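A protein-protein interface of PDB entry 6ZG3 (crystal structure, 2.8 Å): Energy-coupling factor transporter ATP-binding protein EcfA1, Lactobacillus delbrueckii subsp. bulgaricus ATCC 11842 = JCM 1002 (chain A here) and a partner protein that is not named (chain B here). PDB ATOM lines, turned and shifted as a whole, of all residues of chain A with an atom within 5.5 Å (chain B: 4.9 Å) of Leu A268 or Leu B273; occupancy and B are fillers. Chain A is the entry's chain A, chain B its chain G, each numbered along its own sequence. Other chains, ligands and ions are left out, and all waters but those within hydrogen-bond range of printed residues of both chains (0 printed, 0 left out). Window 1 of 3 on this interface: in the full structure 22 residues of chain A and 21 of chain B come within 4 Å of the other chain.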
ATOM      1  N   PRO A 263     -25.487   5.997  15.671  1.00  0.00           N
ATOM      2  CA  PRO A 263     -25.818   5.528  14.320  1.00  0.00           C
ATOM      3  C   PRO A 263     -25.924   4.006  14.236  1.00  0.00           C
ATOM      4  O   PRO A 263     -25.468   3.266  15.114  1.00  0.00           O
ATOM      5  CB  PRO A 263     -24.653   6.055  13.469  1.00  0.00           C
ATOM      6  CG  PRO A 263     -24.117   7.221  14.236  1.00  0.00           C
ATOM      7  CD  PRO A 263     -24.269   6.828  15.676  1.00  0.00           C
ATOM      8  N   PHE A 264     -26.557   3.546  13.149  1.00  0.00           N
ATOM      9  CA  PHE A 264     -26.829   2.120  12.952  1.00  0.00           C
ATOM     10  C   PHE A 264     -25.568   1.268  13.103  1.00  0.00           C
ATOM     11  O   PHE A 264     -25.583   0.248  13.792  1.00  0.00           O
ATOM     12  CB  PHE A 264     -27.472   1.919  11.569  1.00  0.00           C
ATOM     13  CG  PHE A 264     -27.515   0.487  11.094  1.00  0.00           C
ATOM     14  CD1 PHE A 264     -26.424  -0.085  10.453  1.00  0.00           C
ATOM     15  CD2 PHE A 264     -28.662  -0.271  11.241  1.00  0.00           C
ATOM     16  CE1 PHE A 264     -26.464  -1.397  10.024  1.00  0.00           C
ATOM     17  CE2 PHE A 264     -28.706  -1.588  10.805  1.00  0.00           C
ATOM     18  CZ  PHE A 264     -27.615  -2.145  10.199  1.00  0.00           C
ATOM     19  N   VAL A 265     -24.462   1.675  12.481  1.00  0.00           N
ATOM     20  CA  VAL A 265     -23.244   0.867  12.526  1.00  0.00           C
ATOM     21  C   VAL A 265     -22.728   0.729  13.949  1.00  0.00           C
ATOM     22  O   VAL A 265     -22.356  -0.370  14.386  1.00  0.00           O
ATOM     23  CB  VAL A 265     -22.174   1.450  11.589  1.00  0.00           C
ATOM     24  CG1 VAL A 265     -20.786   1.052  12.029  1.00  0.00           C
ATOM     25  CG2 VAL A 265     -22.421   0.951  10.186  1.00  0.00           C
ATOM     26  N   TYR A 266     -22.715   1.821  14.707  1.00  0.00           N
ATOM     27  CA  TYR A 266     -22.187   1.708  16.057  1.00  0.00           C
ATOM     28  C   TYR A 266     -23.117   0.874  16.923  1.00  0.00           C
ATOM     29  O   TYR A 266     -22.664   0.127  17.802  1.00  0.00           O
ATOM     30  CB  TYR A 266     -21.941   3.097  16.634  1.00  0.00           C
ATOM     31  CG  TYR A 266     -21.009   3.949  15.767  1.00  0.00           C
ATOM     32  CD1 TYR A 266     -21.497   4.629  14.646  1.00  0.00           C
ATOM     33  CD2 TYR A 266     -19.642   4.060  16.048  1.00  0.00           C
ATOM     34  CE1 TYR A 266     -20.666   5.400  13.849  1.00  0.00           C
ATOM     35  CE2 TYR A 266     -18.800   4.838  15.243  1.00  0.00           C
ATOM     36  CZ  TYR A 266     -19.326   5.502  14.146  1.00  0.00           C
ATOM     37  OH  TYR A 266     -18.532   6.282  13.333  1.00  0.00           O
ATOM     38  N   ARG A 267     -24.413   0.913  16.630  1.00  0.00           N
ATOM     39  CA  ARG A 267     -25.347   0.053  17.345  1.00  0.00           C
ATOM     40  C   ARG A 267     -25.127  -1.421  17.021  1.00  0.00           C
ATOM     41  O   ARG A 267     -25.102  -2.260  17.925  1.00  0.00           O
ATOM     42  CB  ARG A 267     -26.785   0.474  17.056  1.00  0.00           C
ATOM     43  CG  ARG A 267     -27.721  -0.012  18.133  1.00  0.00           C
ATOM     44  CD  ARG A 267     -27.284   0.563  19.445  1.00  0.00           C
ATOM     45  NE  ARG A 267     -28.395   0.878  20.324  1.00  0.00           N
ATOM     46  CZ  ARG A 267     -28.242   1.278  21.583  1.00  0.00           C
ATOM     47  NH1 ARG A 267     -27.018   1.409  22.086  1.00  0.00           N
ATOM     48  NH2 ARG A 267     -29.302   1.555  22.338  1.00  0.00           N
ATOM     49  N   LEU A 268     -25.012  -1.765  15.738  1.00  0.00           N
ATOM     50  CA  LEU A 268     -24.789  -3.160  15.376  1.00  0.00           C
ATOM     51  C   LEU A 268     -23.494  -3.682  15.980  1.00  0.00           C
ATOM     52  O   LEU A 268     -23.437  -4.818  16.460  1.00  0.00           O
ATOM     53  CB  LEU A 268     -24.766  -3.311  13.860  1.00  0.00           C
ATOM     54  CG  LEU A 268     -24.920  -4.719  13.300  1.00  0.00           C
ATOM     55  CD1 LEU A 268     -26.214  -5.327  13.768  1.00  0.00           C
ATOM     56  CD2 LEU A 268     -24.887  -4.649  11.796  1.00  0.00           C
ATOM     57  N   LYS A 269     -22.446  -2.862  15.969  1.00  0.00           N
ATOM     58  CA  LYS A 269     -21.200  -3.244  16.624  1.00  0.00           C
ATOM     59  C   LYS A 269     -21.423  -3.515  18.108  1.00  0.00           C
ATOM     60  O   LYS A 269     -20.941  -4.519  18.649  1.00  0.00           O
ATOM     61  CB  LYS A 269     -20.144  -2.156  16.417  1.00  0.00           C
ATOM     62  CG  LYS A 269     -19.604  -2.070  14.999  1.00  0.00           C
ATOM     63  CD  LYS A 269     -18.839  -0.786  14.765  1.00  0.00           C
ATOM     64  CE  LYS A 269     -17.750  -0.581  15.801  1.00  0.00           C
ATOM     65  NZ  LYS A 269     -18.194   0.294  16.928  1.00  0.00           N
ATOM     66  N   GLN A 270     -22.149  -2.627  18.791  1.00  0.00           N
ATOM     67  CA  GLN A 270     -22.365  -2.834  20.219  1.00  0.00           C
ATOM     68  C   GLN A 270     -23.164  -4.116  20.472  1.00  0.00           C
ATOM     69  O   GLN A 270     -22.810  -4.915  21.348  1.00  0.00           O
ATOM     70  CB  GLN A 270     -23.064  -1.601  20.834  1.00  0.00           C
ATOM     71  CG  GLN A 270     -23.579  -1.803  22.261  1.00  0.00           C
ATOM     72  CD  GLN A 270     -22.525  -1.484  23.312  1.00  0.00           C
ATOM     73  OE1 GLN A 270     -21.476  -0.929  22.994  1.00  0.00           O
ATOM     74  NE2 GLN A 270     -22.776  -1.887  24.560  1.00  0.00           N
ATOM     75  N   LEU A 271     -24.202  -4.358  19.671  1.00  0.00           N
ATOM     76  CA  LEU A 271     -25.022  -5.557  19.841  1.00  0.00           C
ATOM     77  C   LEU A 271     -24.192  -6.816  19.628  1.00  0.00           C
ATOM     78  O   LEU A 271     -24.238  -7.760  20.431  1.00  0.00           O
ATOM     79  CB  LEU A 271     -26.196  -5.514  18.866  1.00  0.00           C
ATOM     80  CG  LEU A 271     -27.539  -5.065  19.426  1.00  0.00           C
ATOM     81  CD1 LEU A 271     -27.343  -3.708  20.046  1.00  0.00           C
ATOM     82  CD2 LEU A 271     -28.590  -4.989  18.325  1.00  0.00           C
ATOM     83  N   LEU A 272     -23.427  -6.845  18.534  1.00  0.00           N
ATOM     84  CA  LEU A 272     -22.484  -7.928  18.302  1.00  0.00           C
ATOM     85  C   LEU A 272     -21.576  -8.120  19.502  1.00  0.00           C
ATOM     86  O   LEU A 272     -21.225  -9.257  19.849  1.00  0.00           O
ATOM     87  CB  LEU A 272     -21.675  -7.637  17.041  1.00  0.00           C
ATOM     88  CG  LEU A 272     -22.571  -7.768  15.810  1.00  0.00           C
ATOM     89  CD1 LEU A 272     -21.786  -7.581  14.531  1.00  0.00           C
ATOM     90  CD2 LEU A 272     -23.264  -9.127  15.817  1.00  0.00           C
ATOM     91  N   LYS A 273     -21.197  -7.028  20.166  1.00  0.00           N
ATOM     92  CA  LYS A 273     -20.405  -7.194  21.379  1.00  0.00           C
ATOM     93  C   LYS A 273     -21.210  -7.907  22.456  1.00  0.00           C
ATOM     94  O   LYS A 273     -20.715  -8.848  23.092  1.00  0.00           O
ATOM     95  CB  LYS A 273     -19.895  -5.853  21.889  1.00  0.00           C
ATOM     96  CG  LYS A 273     -18.685  -5.977  22.800  1.00  0.00           C
ATOM     97  CD  LYS A 273     -18.276  -4.610  23.328  1.00  0.00           C
ATOM     98  CE  LYS A 273     -16.781  -4.506  23.588  1.00  0.00           C
ATOM     99  NZ  LYS A 273     -16.461  -3.288  24.394  1.00  0.00           N
ATOM    100  N   LEU A 289     -17.630  -2.357   7.643  1.00  0.00           N
ATOM    101  CA  LEU A 289     -18.147  -3.442   8.470  1.00  0.00           C
ATOM    102  C   LEU A 289     -18.429  -4.685   7.642  1.00  0.00           C
ATOM    103  O   LEU A 289     -18.154  -5.810   8.083  1.00  0.00           O
ATOM    104  CB  LEU A 289     -19.408  -2.969   9.199  1.00  0.00           C
ATOM    105  CG  LEU A 289     -20.110  -3.819  10.255  1.00  0.00           C
ATOM    106  CD1 LEU A 289     -19.173  -4.009  11.405  1.00  0.00           C
ATOM    107  CD2 LEU A 289     -21.381  -3.098  10.728  1.00  0.00           C
ATOM    108  N   SER B 249     -31.587  -2.744   8.705  1.00  0.00           N
ATOM    109  CA  SER B 249     -31.014  -4.051   9.047  1.00  0.00           C
ATOM    110  C   SER B 249     -31.280  -5.092   7.968  1.00  0.00           C
ATOM    111  O   SER B 249     -30.454  -5.985   7.757  1.00  0.00           O
ATOM    112  CB  SER B 249     -31.553  -4.533  10.388  1.00  0.00           C
ATOM    113  OG  SER B 249     -31.030  -3.759  11.447  1.00  0.00           O
ATOM    114  N   PHE B 252     -28.679  -4.332   5.456  1.00  0.00           N
ATOM    115  CA  PHE B 252     -27.375  -4.821   5.858  1.00  0.00           C
ATOM    116  C   PHE B 252     -27.314  -6.329   5.727  1.00  0.00           C
ATOM    117  O   PHE B 252     -26.264  -6.890   5.388  1.00  0.00           O
ATOM    118  CB  PHE B 252     -27.058  -4.375   7.270  1.00  0.00           C
ATOM    119  CG  PHE B 252     -25.608  -4.262   7.532  1.00  0.00           C
ATOM    120  CD1 PHE B 252     -24.907  -3.157   7.115  1.00  0.00           C
ATOM    121  CD2 PHE B 252     -24.931  -5.279   8.168  1.00  0.00           C
ATOM    122  CE1 PHE B 252     -23.546  -3.054   7.352  1.00  0.00           C
ATOM    123  CE2 PHE B 252     -23.573  -5.191   8.403  1.00  0.00           C
ATOM    124  CZ  PHE B 252     -22.881  -4.078   7.994  1.00  0.00           C
ATOM    125  N   ALA B 253     -28.437  -7.000   5.970  1.00  0.00           N
ATOM    126  CA  ALA B 253     -28.538  -8.411   5.631  1.00  0.00           C
ATOM    127  C   ALA B 253     -28.242  -8.632   4.159  1.00  0.00           C
ATOM    128  O   ALA B 253     -27.446  -9.496   3.803  1.00  0.00           O
ATOM    129  CB  ALA B 253     -29.932  -8.940   5.974  1.00  0.00           C
ATOM    130  N   LEU B 256     -24.466  -8.059   3.357  1.00  0.00           N
ATOM    131  CA  LEU B 256     -23.690  -9.223   3.772  1.00  0.00           C
ATOM    132  C   LEU B 256     -23.968 -10.427   2.877  1.00  0.00           C
ATOM    133  O   LEU B 256     -23.049 -11.179   2.556  1.00  0.00           O
ATOM    134  CB  LEU B 256     -23.979  -9.542   5.237  1.00  0.00           C
ATOM    135  CG  LEU B 256     -23.485  -8.504   6.248  1.00  0.00           C
ATOM    136  CD1 LEU B 256     -23.989  -8.827   7.643  1.00  0.00           C
ATOM    137  CD2 LEU B 256     -21.969  -8.441   6.254  1.00  0.00           C
ATOM    138  N   LEU B 263     -26.405 -15.798   6.356  1.00  0.00           N
ATOM    139  CA  LEU B 263     -27.273 -15.294   7.421  1.00  0.00           C
ATOM    140  C   LEU B 263     -28.596 -16.044   7.454  1.00  0.00           C
ATOM    141  O   LEU B 263     -29.303 -16.086   6.437  1.00  0.00           O
ATOM    142  CB  LEU B 263     -27.527 -13.793   7.275  1.00  0.00           C
ATOM    143  CG  LEU B 263     -26.592 -12.857   8.050  1.00  0.00           C
ATOM    144  CD1 LEU B 263     -25.137 -13.195   7.863  1.00  0.00           C
ATOM    145  CD2 LEU B 263     -26.862 -11.413   7.693  1.00  0.00           C
ATOM    146  N   PRO B 267     -33.561 -11.556   8.759  1.00  0.00           N
ATOM    147  CA  PRO B 267     -33.358 -10.560   9.819  1.00  0.00           C
ATOM    148  C   PRO B 267     -33.902  -9.202   9.385  1.00  0.00           C
ATOM    149  O   PRO B 267     -33.538  -8.676   8.330  1.00  0.00           O
ATOM    150  CB  PRO B 267     -31.832 -10.539  10.006  1.00  0.00           C
ATOM    151  CG  PRO B 267     -31.279 -11.025   8.728  1.00  0.00           C
ATOM    152  CD  PRO B 267     -32.319 -11.865   8.029  1.00  0.00           C
ATOM    153  N   THR B 269     -34.889  -6.775  12.318  1.00  0.00           N
ATOM    154  CA  THR B 269     -34.494  -5.913  13.422  1.00  0.00           C
ATOM    155  C   THR B 269     -32.994  -5.984  13.637  1.00  0.00           C
ATOM    156  O   THR B 269     -32.314  -6.882  13.138  1.00  0.00           O
ATOM    157  CB  THR B 269     -35.181  -6.307  14.725  1.00  0.00           C
ATOM    158  OG1 THR B 269     -36.141  -7.349  14.489  1.00  0.00           O
ATOM    159  CG2 THR B 269     -35.845  -5.093  15.327  1.00  0.00           C
ATOM    160  N   MET B 270     -32.469  -4.998  14.353  1.00  0.00           N
ATOM    161  CA  MET B 270     -31.053  -5.052  14.699  1.00  0.00           C
ATOM    162  C   MET B 270     -30.725  -6.236  15.587  1.00  0.00           C
ATOM    163  O   MET B 270     -29.701  -6.892  15.337  1.00  0.00           O
ATOM    164  CB  MET B 270     -30.605  -3.741  15.328  1.00  0.00           C
ATOM    165  CG  MET B 270     -30.738  -2.594  14.376  1.00  0.00           C
ATOM    166  SD  MET B 270     -29.374  -1.470  14.624  1.00  0.00           S
ATOM    167  CE  MET B 270     -30.144  -0.243  15.679  1.00  0.00           C
ATOM    168  N   PRO B 271     -31.498  -6.558  16.638  1.00  0.00           N
ATOM    169  CA  PRO B 271     -31.202  -7.802  17.363  1.00  0.00           C
ATOM    170  C   PRO B 271     -31.232  -9.033  16.478  1.00  0.00           C
ATOM    171  O   PRO B 271     -30.278  -9.813  16.512  1.00  0.00           O
ATOM    172  CB  PRO B 271     -32.287  -7.832  18.437  1.00  0.00           C
ATOM    173  CG  PRO B 271     -32.534  -6.436  18.714  1.00  0.00           C
ATOM    174  CD  PRO B 271     -32.470  -5.742  17.386  1.00  0.00           C
ATOM    175  N   GLU B 272     -32.281  -9.226  15.676  1.00  0.00           N
ATOM    176  CA  GLU B 272     -32.308 -10.397  14.803  1.00  0.00           C
ATOM    177  C   GLU B 272     -31.097 -10.426  13.883  1.00  0.00           C
ATOM    178  O   GLU B 272     -30.521 -11.489  13.635  1.00  0.00           O
ATOM    179  CB  GLU B 272     -33.590 -10.430  13.983  1.00  0.00           C
ATOM    180  CG  GLU B 272     -34.814 -10.801  14.765  1.00  0.00           C
ATOM    181  CD  GLU B 272     -36.081 -10.490  13.995  1.00  0.00           C
ATOM    182  OE1 GLU B 272     -36.089 -10.678  12.766  1.00  0.00           O
ATOM    183  OE2 GLU B 272     -37.071 -10.047  14.615  1.00  0.00           O
ATOM    184  N   LEU B 273     -30.699  -9.260  13.375  1.00  0.00           N
ATOM    185  CA  LEU B 273     -29.529  -9.169  12.510  1.00  0.00           C
ATOM    186  C   LEU B 273     -28.255  -9.567  13.252  1.00  0.00           C
ATOM    187  O   LEU B 273     -27.444 -10.345  12.736  1.00  0.00           O
ATOM    188  CB  LEU B 273     -29.422  -7.752  11.946  1.00  0.00           C
ATOM    189  CG  LEU B 273     -28.117  -7.404  11.233  1.00  0.00           C
ATOM    190  CD1 LEU B 273     -27.822  -8.401  10.093  1.00  0.00           C
ATOM    191  CD2 LEU B 273     -28.153  -5.972  10.716  1.00  0.00           C
ATOM    192  N   ALA B 274     -28.049  -9.023  14.457  1.00  0.00           N
ATOM    193  CA  ALA B 274     -26.866  -9.373  15.241  1.00  0.00           C
ATOM    194  C   ALA B 274     -26.856 -10.866  15.557  1.00  0.00           C
ATOM    195  O   ALA B 274     -25.809 -11.527  15.495  1.00  0.00           O
ATOM    196  CB  ALA B 274     -26.820  -8.544  16.526  1.00  0.00           C
ATOM    197  N   ASP B 275     -28.020 -11.411  15.901  1.00  0.00           N
ATOM    198  CA  ASP B 275     -28.138 -12.844  16.129  1.00  0.00           C
ATOM    199  C   ASP B 275     -27.712 -13.639  14.901  1.00  0.00           C
ATOM    200  O   ASP B 275     -26.887 -14.554  15.001  1.00  0.00           O
ATOM    201  CB  ASP B 275     -29.571 -13.186  16.534  1.00  0.00           C
ATOM    202  CG  ASP B 275     -29.926 -12.619  17.885  1.00  0.00           C
ATOM    203  OD1 ASP B 275     -28.969 -12.283  18.626  1.00  0.00           O
ATOM    204  OD2 ASP B 275     -31.139 -12.520  18.206  1.00  0.00           O
ATOM    205  N   ALA B 276     -28.274 -13.313  13.735  1.00  0.00           N
ATOM    206  CA  ALA B 276     -27.947 -14.066  12.530  1.00  0.00           C
ATOM    207  C   ALA B 276     -26.474 -13.921  12.169  1.00  0.00           C
ATOM    208  O   ALA B 276     -25.881 -14.850  11.617  1.00  0.00           O
ATOM    209  CB  ALA B 276     -28.836 -13.612  11.374  1.00  0.00           C
ATOM    210  N   ILE B 277     -25.865 -12.779  12.491  1.00  0.00           N
ATOM    211  CA  ILE B 277     -24.431 -12.618  12.273  1.00  0.00           C
ATOM    212  C   ILE B 277     -23.655 -13.558  13.183  1.00  0.00           C
ATOM    213  O   ILE B 277     -22.713 -14.232  12.750  1.00  0.00           O
ATOM    214  CB  ILE B 277     -24.023 -11.149  12.489  1.00  0.00           C
ATOM    215  CG1 ILE B 277     -24.481 -10.287  11.302  1.00  0.00           C
ATOM    216  CG2 ILE B 277     -22.530 -11.035  12.766  1.00  0.00           C
ATOM    217  CD1 ILE B 277     -24.554  -8.799  11.618  1.00  0.00           C
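Of chain B, only Phe B252 and Leu B273 come within 4 Å of Leu A268. Printed residues of chain A within 4 Å of Leu B273: Phe A264 and Leu A268. Of the printed residues of chain A, Met B270 touches Phe A264 (3.7 Å), Arg A267 (3.5 Å) and Leu A271 (3.7 Å). Of the printed residues of chain A, Ser B249 touches Phe A264. Ala B276 touches none of the printed residues of chain A. The nearest residue of chain B that does not touch Leu A268 is Met B270 (4.1 Å).
N of Met B270 lies close to OG of Ser B249 (3.5 Å).
Among the printed residues, 13 pairs touch across the chains.
Phe A264 touches Met B270. Phe A264 touches Leu B273. Met B270 touches Arg A267 (CE to CG, 3.5 Å). Leu A268 touches Phe B252. CD2 of Leu A271 touches C of Met B270, 3.7 Å away. Pro B271 touches Leu A271 (N to CD2, 3.7 Å). Ala B274 touches Leu A271 (CB to CB, 3.9 Å). CD2 of Leu A272 touches O of Ala B274, at 3.5 Å. CD2 of Leu A272 touches CG2 of Ile B277 (3.7 Å). CD2 of Leu A289 touches CZ of Phe B252 (3.3 Å).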
